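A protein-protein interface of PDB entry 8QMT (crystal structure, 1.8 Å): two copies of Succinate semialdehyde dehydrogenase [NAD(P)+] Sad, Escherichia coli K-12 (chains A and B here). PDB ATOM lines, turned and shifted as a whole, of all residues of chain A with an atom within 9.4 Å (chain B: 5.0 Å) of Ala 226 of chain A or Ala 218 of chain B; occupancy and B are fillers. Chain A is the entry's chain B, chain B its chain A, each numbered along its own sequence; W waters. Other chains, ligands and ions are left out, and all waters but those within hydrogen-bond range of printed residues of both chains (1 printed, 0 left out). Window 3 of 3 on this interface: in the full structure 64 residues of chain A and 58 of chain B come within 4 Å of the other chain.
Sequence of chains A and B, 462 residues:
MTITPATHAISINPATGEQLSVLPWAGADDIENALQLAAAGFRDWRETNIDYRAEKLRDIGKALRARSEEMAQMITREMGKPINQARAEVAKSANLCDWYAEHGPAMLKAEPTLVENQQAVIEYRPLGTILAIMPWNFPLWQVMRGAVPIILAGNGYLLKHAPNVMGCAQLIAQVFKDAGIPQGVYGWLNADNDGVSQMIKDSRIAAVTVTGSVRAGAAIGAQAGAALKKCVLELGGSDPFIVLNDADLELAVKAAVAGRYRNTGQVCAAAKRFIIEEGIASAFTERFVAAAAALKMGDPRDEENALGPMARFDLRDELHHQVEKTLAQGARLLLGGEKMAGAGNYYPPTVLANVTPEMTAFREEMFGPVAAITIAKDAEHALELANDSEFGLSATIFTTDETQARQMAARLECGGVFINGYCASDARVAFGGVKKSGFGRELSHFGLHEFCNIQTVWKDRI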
ATOM      1  N   SER A 197      17.033  30.060 -26.895  1.00  0.00           N
ATOM      2  CA  SER A 197      16.570  29.301 -25.735  1.00  0.00           C
ATOM      3  C   SER A 197      15.347  28.474 -26.091  1.00  0.00           C
ATOM      4  O   SER A 197      15.228  27.307 -25.697  1.00  0.00           O
ATOM      5  CB  SER A 197      16.236  30.246 -24.578  1.00  0.00           C
ATOM      6  OG  SER A 197      17.366  30.980 -24.157  1.00  0.00           O
ATOM      7  N   ILE A 200      16.417  25.423 -28.334  1.00  0.00           N
ATOM      8  CA  ILE A 200      17.094  24.372 -27.573  1.00  0.00           C
ATOM      9  C   ILE A 200      16.079  23.467 -26.874  1.00  0.00           C
ATOM     10  O   ILE A 200      16.230  22.233 -26.839  1.00  0.00           O
ATOM     11  CB  ILE A 200      18.085  25.007 -26.578  1.00  0.00           C
ATOM     12  CG1 ILE A 200      19.246  25.651 -27.340  1.00  0.00           C
ATOM     13  CG2 ILE A 200      18.571  23.967 -25.554  1.00  0.00           C
ATOM     14  CD1 ILE A 200      20.140  26.531 -26.474  1.00  0.00           C
ATOM     15  N   LYS A 201      15.003  24.057 -26.346  1.00  0.00           N
ATOM     16  CA  LYS A 201      13.962  23.295 -25.658  1.00  0.00           C
ATOM     17  C   LYS A 201      13.017  22.546 -26.596  1.00  0.00           C
ATOM     18  O   LYS A 201      12.197  21.755 -26.111  1.00  0.00           O
ATOM     19  CB  LYS A 201      13.117  24.220 -24.776  1.00  0.00           C
ATOM     20  CG  LYS A 201      13.838  24.806 -23.576  1.00  0.00           C
ATOM     21  CD  LYS A 201      12.833  25.461 -22.633  1.00  0.00           C
ATOM     22  CE  LYS A 201      13.168  26.914 -22.361  1.00  0.00           C
ATOM     23  NZ  LYS A 201      13.262  27.167 -20.894  1.00  0.00           N
ATOM     24  N   VAL A 208      23.214  20.527 -30.276  1.00  0.00           N
ATOM     25  CA  VAL A 208      23.647  21.915 -30.394  1.00  0.00           C
ATOM     26  C   VAL A 208      25.160  21.940 -30.556  1.00  0.00           C
ATOM     27  O   VAL A 208      25.882  21.192 -29.888  1.00  0.00           O
ATOM     28  CB  VAL A 208      23.237  22.758 -29.166  1.00  0.00           C
ATOM     29  CG1 VAL A 208      23.435  24.240 -29.445  1.00  0.00           C
ATOM     30  CG2 VAL A 208      21.786  22.467 -28.746  1.00  0.00           C
ATOM     31  N   ALA A 218      28.972  28.664 -21.814  1.00  0.00           N
ATOM     32  CA  ALA A 218      28.394  28.298 -20.526  1.00  0.00           C
ATOM     33  C   ALA A 218      26.886  28.520 -20.515  1.00  0.00           C
ATOM     34  O   ALA A 218      26.135  27.688 -19.994  1.00  0.00           O
ATOM     35  CB  ALA A 218      29.070  29.090 -19.405  1.00  0.00           C
ATOM     36  N   ALA A 219      26.427  29.624 -21.106  1.00  0.00           N
ATOM     37  CA  ALA A 219      24.996  29.900 -21.177  1.00  0.00           C
ATOM     38  C   ALA A 219      24.281  28.867 -22.035  1.00  0.00           C
ATOM     39  O   ALA A 219      23.225  28.352 -21.653  1.00  0.00           O
ATOM     40  CB  ALA A 219      24.756  31.312 -21.726  1.00  0.00           C
ATOM     41  N   ILE A 220      24.841  28.549 -23.202  1.00  0.00           N
ATOM     42  CA  ILE A 220      24.170  27.619 -24.104  1.00  0.00           C
ATOM     43  C   ILE A 220      24.356  26.180 -23.641  1.00  0.00           C
ATOM     44  O   ILE A 220      23.424  25.373 -23.708  1.00  0.00           O
ATOM     45  CB  ILE A 220      24.677  27.817 -25.541  1.00  0.00           C
ATOM     46  CG1 ILE A 220      24.243  29.184 -26.061  1.00  0.00           C
ATOM     47  CG2 ILE A 220      24.121  26.719 -26.438  1.00  0.00           C
ATOM     48  CD1 ILE A 220      25.165  29.745 -27.160  1.00  0.00           C
ATOM     49  N   GLY A 221      25.554  25.825 -23.173  1.00  0.00           N
ATOM     50  CA  GLY A 221      25.758  24.470 -22.680  1.00  0.00           C
ATOM     51  C   GLY A 221      24.840  24.120 -21.523  1.00  0.00           C
ATOM     52  O   GLY A 221      24.341  22.997 -21.432  1.00  0.00           O
ATOM     53  N   ALA A 222      24.622  25.066 -20.608  1.00  0.00           N
ATOM     54  CA  ALA A 222      23.701  24.817 -19.502  1.00  0.00           C
ATOM     55  C   ALA A 222      22.291  24.544 -20.009  1.00  0.00           C
ATOM     56  O   ALA A 222      21.577  23.686 -19.470  1.00  0.00           O
ATOM     57  CB  ALA A 222      23.700  26.007 -18.548  1.00  0.00           C
ATOM     58  N   GLN A 223      21.864  25.276 -21.039  1.00  0.00           N
ATOM     59  CA  GLN A 223      20.522  25.064 -21.576  1.00  0.00           C
ATOM     60  C   GLN A 223      20.424  23.740 -22.315  1.00  0.00           C
ATOM     61  O   GLN A 223      19.402  23.047 -22.226  1.00  0.00           O
ATOM     62  CB  GLN A 223      20.139  26.214 -22.500  1.00  0.00           C
ATOM     63  CG  GLN A 223      20.072  27.539 -21.791  1.00  0.00           C
ATOM     64  CD  GLN A 223      19.700  28.655 -22.746  1.00  0.00           C
ATOM     65  OE1 GLN A 223      18.549  28.756 -23.172  1.00  0.00           O
ATOM     66  NE2 GLN A 223      20.675  29.487 -23.103  1.00  0.00           N
ATOM     67  N   ALA A 224      21.464  23.384 -23.074  1.00  0.00           N
ATOM     68  CA  ALA A 224      21.470  22.095 -23.757  1.00  0.00           C
ATOM     69  C   ALA A 224      21.384  20.945 -22.758  1.00  0.00           C
ATOM     70  O   ALA A 224      20.587  20.017 -22.930  1.00  0.00           O
ATOM     71  CB  ALA A 224      22.725  21.970 -24.629  1.00  0.00           C
ATOM     72  N   GLY A 225      22.194  20.995 -21.697  1.00  0.00           N
ATOM     73  CA  GLY A 225      22.125  19.955 -20.678  1.00  0.00           C
ATOM     74  C   GLY A 225      20.760  19.864 -20.022  1.00  0.00           C
ATOM     75  O   GLY A 225      20.236  18.767 -19.800  1.00  0.00           O
ATOM     76  N   ALA A 226      20.153  21.015 -19.718  1.00  0.00           N
ATOM     77  CA  ALA A 226      18.835  21.005 -19.087  1.00  0.00           C
ATOM     78  C   ALA A 226      17.774  20.418 -20.005  1.00  0.00           C
ATOM     79  O   ALA A 226      16.793  19.843 -19.526  1.00  0.00           O
ATOM     80  CB  ALA A 226      18.438  22.425 -18.668  1.00  0.00           C
ATOM     81  N   ALA A 227      17.943  20.558 -21.321  1.00  0.00           N
ATOM     82  CA  ALA A 227      17.015  20.004 -22.296  1.00  0.00           C
ATOM     83  C   ALA A 227      17.414  18.608 -22.771  1.00  0.00           C
ATOM     84  O   ALA A 227      16.771  18.064 -23.677  1.00  0.00           O
ATOM     85  CB  ALA A 227      16.880  20.946 -23.495  1.00  0.00           C
ATOM     86  N   LEU A 228      18.456  18.023 -22.178  1.00  0.00           N
ATOM     87  CA  LEU A 228      18.924  16.676 -22.524  1.00  0.00           C
ATOM     88  C   LEU A 228      19.385  16.605 -23.981  1.00  0.00           C
ATOM     89  O   LEU A 228      19.145  15.619 -24.681  1.00  0.00           O
ATOM     90  CB  LEU A 228      17.852  15.623 -22.223  1.00  0.00           C
ATOM     91  CG  LEU A 228      17.381  15.613 -20.769  1.00  0.00           C
ATOM     92  CD1 LEU A 228      16.375  14.485 -20.550  1.00  0.00           C
ATOM     93  CD2 LEU A 228      18.586  15.458 -19.853  1.00  0.00           C
ATOM     94  N   LYS A 229      20.065  17.661 -24.433  1.00  0.00           N
ATOM     95  CA  LYS A 229      20.606  17.765 -25.786  1.00  0.00           C
ATOM     96  C   LYS A 229      22.129  17.722 -25.712  1.00  0.00           C
ATOM     97  O   LYS A 229      22.736  18.497 -24.964  1.00  0.00           O
ATOM     98  CB  LYS A 229      20.181  19.071 -26.474  1.00  0.00           C
ATOM     99  CG  LYS A 229      18.680  19.425 -26.451  1.00  0.00           C
ATOM    100  CD  LYS A 229      17.861  18.450 -27.273  1.00  0.00           C
ATOM    101  CE  LYS A 229      16.363  18.663 -27.065  1.00  0.00           C
ATOM    102  NZ  LYS A 229      15.771  19.675 -27.998  1.00  0.00           N
ATOM    103  N   LYS A 230      22.748  16.830 -26.484  1.00  0.00           N
ATOM    104  CA  LYS A 230      24.209  16.823 -26.560  1.00  0.00           C
ATOM    105  C   LYS A 230      24.705  18.124 -27.171  1.00  0.00           C
ATOM    106  O   LYS A 230      24.079  18.677 -28.082  1.00  0.00           O
ATOM    107  CB  LYS A 230      24.701  15.642 -27.396  1.00  0.00           C
ATOM    108  CG  LYS A 230      26.210  15.591 -27.566  1.00  0.00           C
ATOM    109  CD  LYS A 230      26.660  14.351 -28.336  1.00  0.00           C
ATOM    110  CE  LYS A 230      28.130  14.472 -28.720  1.00  0.00           C
ATOM    111  NZ  LYS A 230      28.651  13.275 -29.437  1.00  0.00           N
ATOM    112  N   CYS A 231      25.837  18.625 -26.668  1.00  0.00           N
ATOM    113  CA  CYS A 231      26.432  19.805 -27.279  1.00  0.00           C
ATOM    114  C   CYS A 231      27.917  19.585 -27.519  1.00  0.00           C
ATOM    115  O   CYS A 231      28.564  18.763 -26.862  1.00  0.00           O
ATOM    116  CB  CYS A 231      26.203  21.087 -26.441  1.00  0.00           C
ATOM    117  SG  CYS A 231      26.965  21.092 -24.814  1.00  0.00           S
ATOM    118  N   VAL B 214      15.569  10.764 -15.869  1.00  0.00           N
ATOM    119  CA  VAL B 214      15.575  11.919 -16.755  1.00  0.00           C
ATOM    120  C   VAL B 214      15.762  13.197 -15.952  1.00  0.00           C
ATOM    121  O   VAL B 214      16.535  14.085 -16.333  1.00  0.00           O
ATOM    122  CB  VAL B 214      14.270  11.937 -17.575  1.00  0.00           C
ATOM    123  CG1 VAL B 214      14.081  13.272 -18.252  1.00  0.00           C
ATOM    124  CG2 VAL B 214      14.279  10.810 -18.592  1.00  0.00           C
ATOM    125  N   ARG B 215      15.074  13.295 -14.811  1.00  0.00           N
ATOM    126  CA  ARG B 215      15.174  14.477 -13.957  1.00  0.00           C
ATOM    127  C   ARG B 215      16.601  14.682 -13.446  1.00  0.00           C
ATOM    128  O   ARG B 215      17.094  15.816 -13.395  1.00  0.00           O
ATOM    129  CB  ARG B 215      14.181  14.326 -12.796  1.00  0.00           C
ATOM    130  CG  ARG B 215      14.118  15.473 -11.805  1.00  0.00           C
ATOM    131  CD  ARG B 215      13.170  15.124 -10.644  1.00  0.00           C
ATOM    132  NE  ARG B 215      13.200  16.132  -9.588  1.00  0.00           N
ATOM    133  CZ  ARG B 215      12.579  16.025  -8.419  1.00  0.00           C
ATOM    134  NH1 ARG B 215      11.855  14.958  -8.113  1.00  0.00           N
ATOM    135  NH2 ARG B 215      12.691  17.013  -7.533  1.00  0.00           N
ATOM    136  N   ALA B 216      17.279  13.596 -13.070  1.00  0.00           N
ATOM    137  CA  ALA B 216      18.664  13.694 -12.612  1.00  0.00           C
ATOM    138  C   ALA B 216      19.597  14.119 -13.742  1.00  0.00           C
ATOM    139  O   ALA B 216      20.479  14.970 -13.552  1.00  0.00           O
ATOM    140  CB  ALA B 216      19.114  12.350 -12.035  1.00  0.00           C
ATOM    141  N   GLY B 217      19.427  13.529 -14.924  1.00  0.00           N
ATOM    142  CA  GLY B 217      20.266  13.905 -16.048  1.00  0.00           C
ATOM    143  C   GLY B 217      20.094  15.359 -16.449  1.00  0.00           C
ATOM    144  O   GLY B 217      21.062  16.029 -16.811  1.00  0.00           O
ATOM    145  N   ALA B 218      18.862  15.870 -16.384  1.00  0.00           N
ATOM    146  CA  ALA B 218      18.638  17.275 -16.719  1.00  0.00           C
ATOM    147  C   ALA B 218      19.270  18.197 -15.682  1.00  0.00           C
ATOM    148  O   ALA B 218      19.907  19.202 -16.038  1.00  0.00           O
ATOM    149  CB  ALA B 218      17.139  17.555 -16.856  1.00  0.00           C
ATOM    150  N   ALA B 219      19.131  17.864 -14.396  1.00  0.00           N
ATOM    151  CA  ALA B 219      19.726  18.698 -13.353  1.00  0.00           C
ATOM    152  C   ALA B 219      21.246  18.672 -13.420  1.00  0.00           C
ATOM    153  O   ALA B 219      21.896  19.715 -13.291  1.00  0.00           O
ATOM    154  CB  ALA B 219      19.254  18.244 -11.973  1.00  0.00           C
ATOM    155  N   ILE B 220      21.834  17.492 -13.605  1.00  0.00           N
ATOM    156  CA  ILE B 220      23.290  17.398 -13.614  1.00  0.00           C
ATOM    157  C   ILE B 220      23.854  17.898 -14.940  1.00  0.00           C
ATOM    158  O   ILE B 220      24.855  18.629 -14.967  1.00  0.00           O
ATOM    159  CB  ILE B 220      23.719  15.949 -13.308  1.00  0.00           C
ATOM    160  CG1 ILE B 220      23.316  15.568 -11.879  1.00  0.00           C
ATOM    161  CG2 ILE B 220      25.221  15.798 -13.467  1.00  0.00           C
ATOM    162  CD1 ILE B 220      23.279  14.070 -11.620  1.00  0.00           C
ATOM    163  N   GLY B 221      23.213  17.532 -16.061  1.00  0.00           N
ATOM    164  CA  GLY B 221      23.696  17.983 -17.360  1.00  0.00           C
ATOM    165  C   GLY B 221      23.720  19.497 -17.479  1.00  0.00           C
ATOM    166  O   GLY B 221      24.645  20.076 -18.065  1.00  0.00           O
ATOM    167  N   ALA B 222      22.707  20.160 -16.920  1.00  0.00           N
ATOM    168  CA  ALA B 222      22.699  21.622 -16.919  1.00  0.00           C
ATOM    169  C   ALA B 222      23.893  22.178 -16.151  1.00  0.00           C
ATOM    170  O   ALA B 222      24.508  23.174 -16.566  1.00  0.00           O
ATOM    171  CB  ALA B 222      21.389  22.139 -16.318  1.00  0.00           C
ATOM    172  N   LEU B 235      19.691   7.813 -19.321  1.00  0.00           N
ATOM    173  CA  LEU B 235      18.569   8.174 -18.412  1.00  0.00           C
ATOM    174  C   LEU B 235      17.335   7.278 -18.545  1.00  0.00           C
ATOM    175  O   LEU B 235      16.233   7.755 -18.297  1.00  0.00           O
ATOM    176  CB  LEU B 235      18.242   9.639 -18.713  1.00  0.00           C
ATOM    177  CG  LEU B 235      19.452  10.567 -18.763  1.00  0.00           C
ATOM    178  CD1 LEU B 235      19.029  11.988 -19.075  1.00  0.00           C
ATOM    179  CD2 LEU B 235      20.228  10.512 -17.459  1.00  0.00           C
HETATM  180  O   HOH W   1      25.200  20.207 -21.068  1.00  0.00           O
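CA of Ala 222 of chain A touches O of Ala 222 of chain B (3.5 Å). Ala 218 of chain B touches Gly 225 of chain A. Gly 225 of chain A touches Gly 221 of chain B (CA to C, 3.6 Å). C of Gly 225 of chain A touches N of Ala 222 of chain B (3.7 Å). Ala 218 of chain B touches Ala 226 of chain A (CB to O, 3.5 Å). Ala 222 of chain B touches Ala 226 of chain A. CD1 of Leu 228 of chain A touches CG1 of Val 214 of chain B, 3.5 Å away. Gly 217 of chain B touches Leu 228 of chain A (C to CD2, 3.7 Å). N of Ala 218 of chain B touches CD2 of Leu 228 of chain A, at 3.5 Å. CD1 of Leu 235 of chain B touches CD2 of Leu 228 of chain A (3.6 Å).
Of the printed residues of chain B, Ala 222 of chain A touches Ala 222. Of the printed residues of chain A, Val 214 of chain B touches Leu 228. Arg 215 of chain B touches none of the printed residues of chain A. Ala 218 of chain B touches just these residues of chain A: Gly 225, Ala 226 and Leu 228. No residue of chain A comes within 4 Å of Ala 219 of chain B. Gly 221 of chain B touches one residue of chain A. Of the printed residues of chain A, Ala 222 of chain B touches Ala 222, Gly 225 and Ala 226. The nearest residue of chain B that does not touch Ala 226 of chain A is Gly 221 of chain B (4.5 Å). The nearest printed residue of chain A that does not touch Leu 235 of chain B is Gly 225 of chain A (6.9 Å).
Of the 18 printed residues of chain A, 4 touch a printed residue of chain B. Printed residues of chain A that touch a printed residue of chain B: Ala 222, Gly 225, Ala 226 and Leu 228. Along chain A the printed residues that touch a printed residue of chain B span positions 222 to 228. Hydrophobic or aromatic side chains of chain B that line the printed part of chain A: Val 214, Ala 218, Ala 222 and Leu 235.
Ala 222 of chain A touches its own counterpart, Ala 222 of chain B. Positions printed for both chains: 218, 219, 220, 221 and 222. Of the 10 pairs that touch across the chains among the printed residues, 1 has its exchanged pair printed and touching as well.
Water W1 lies within hydrogen-bond range of O of Gly 221 of chain A (2.9 Å), O of Gly 221 of chain B (3.1 Å) and N of Gly 225 of chain A (3.2 Å).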
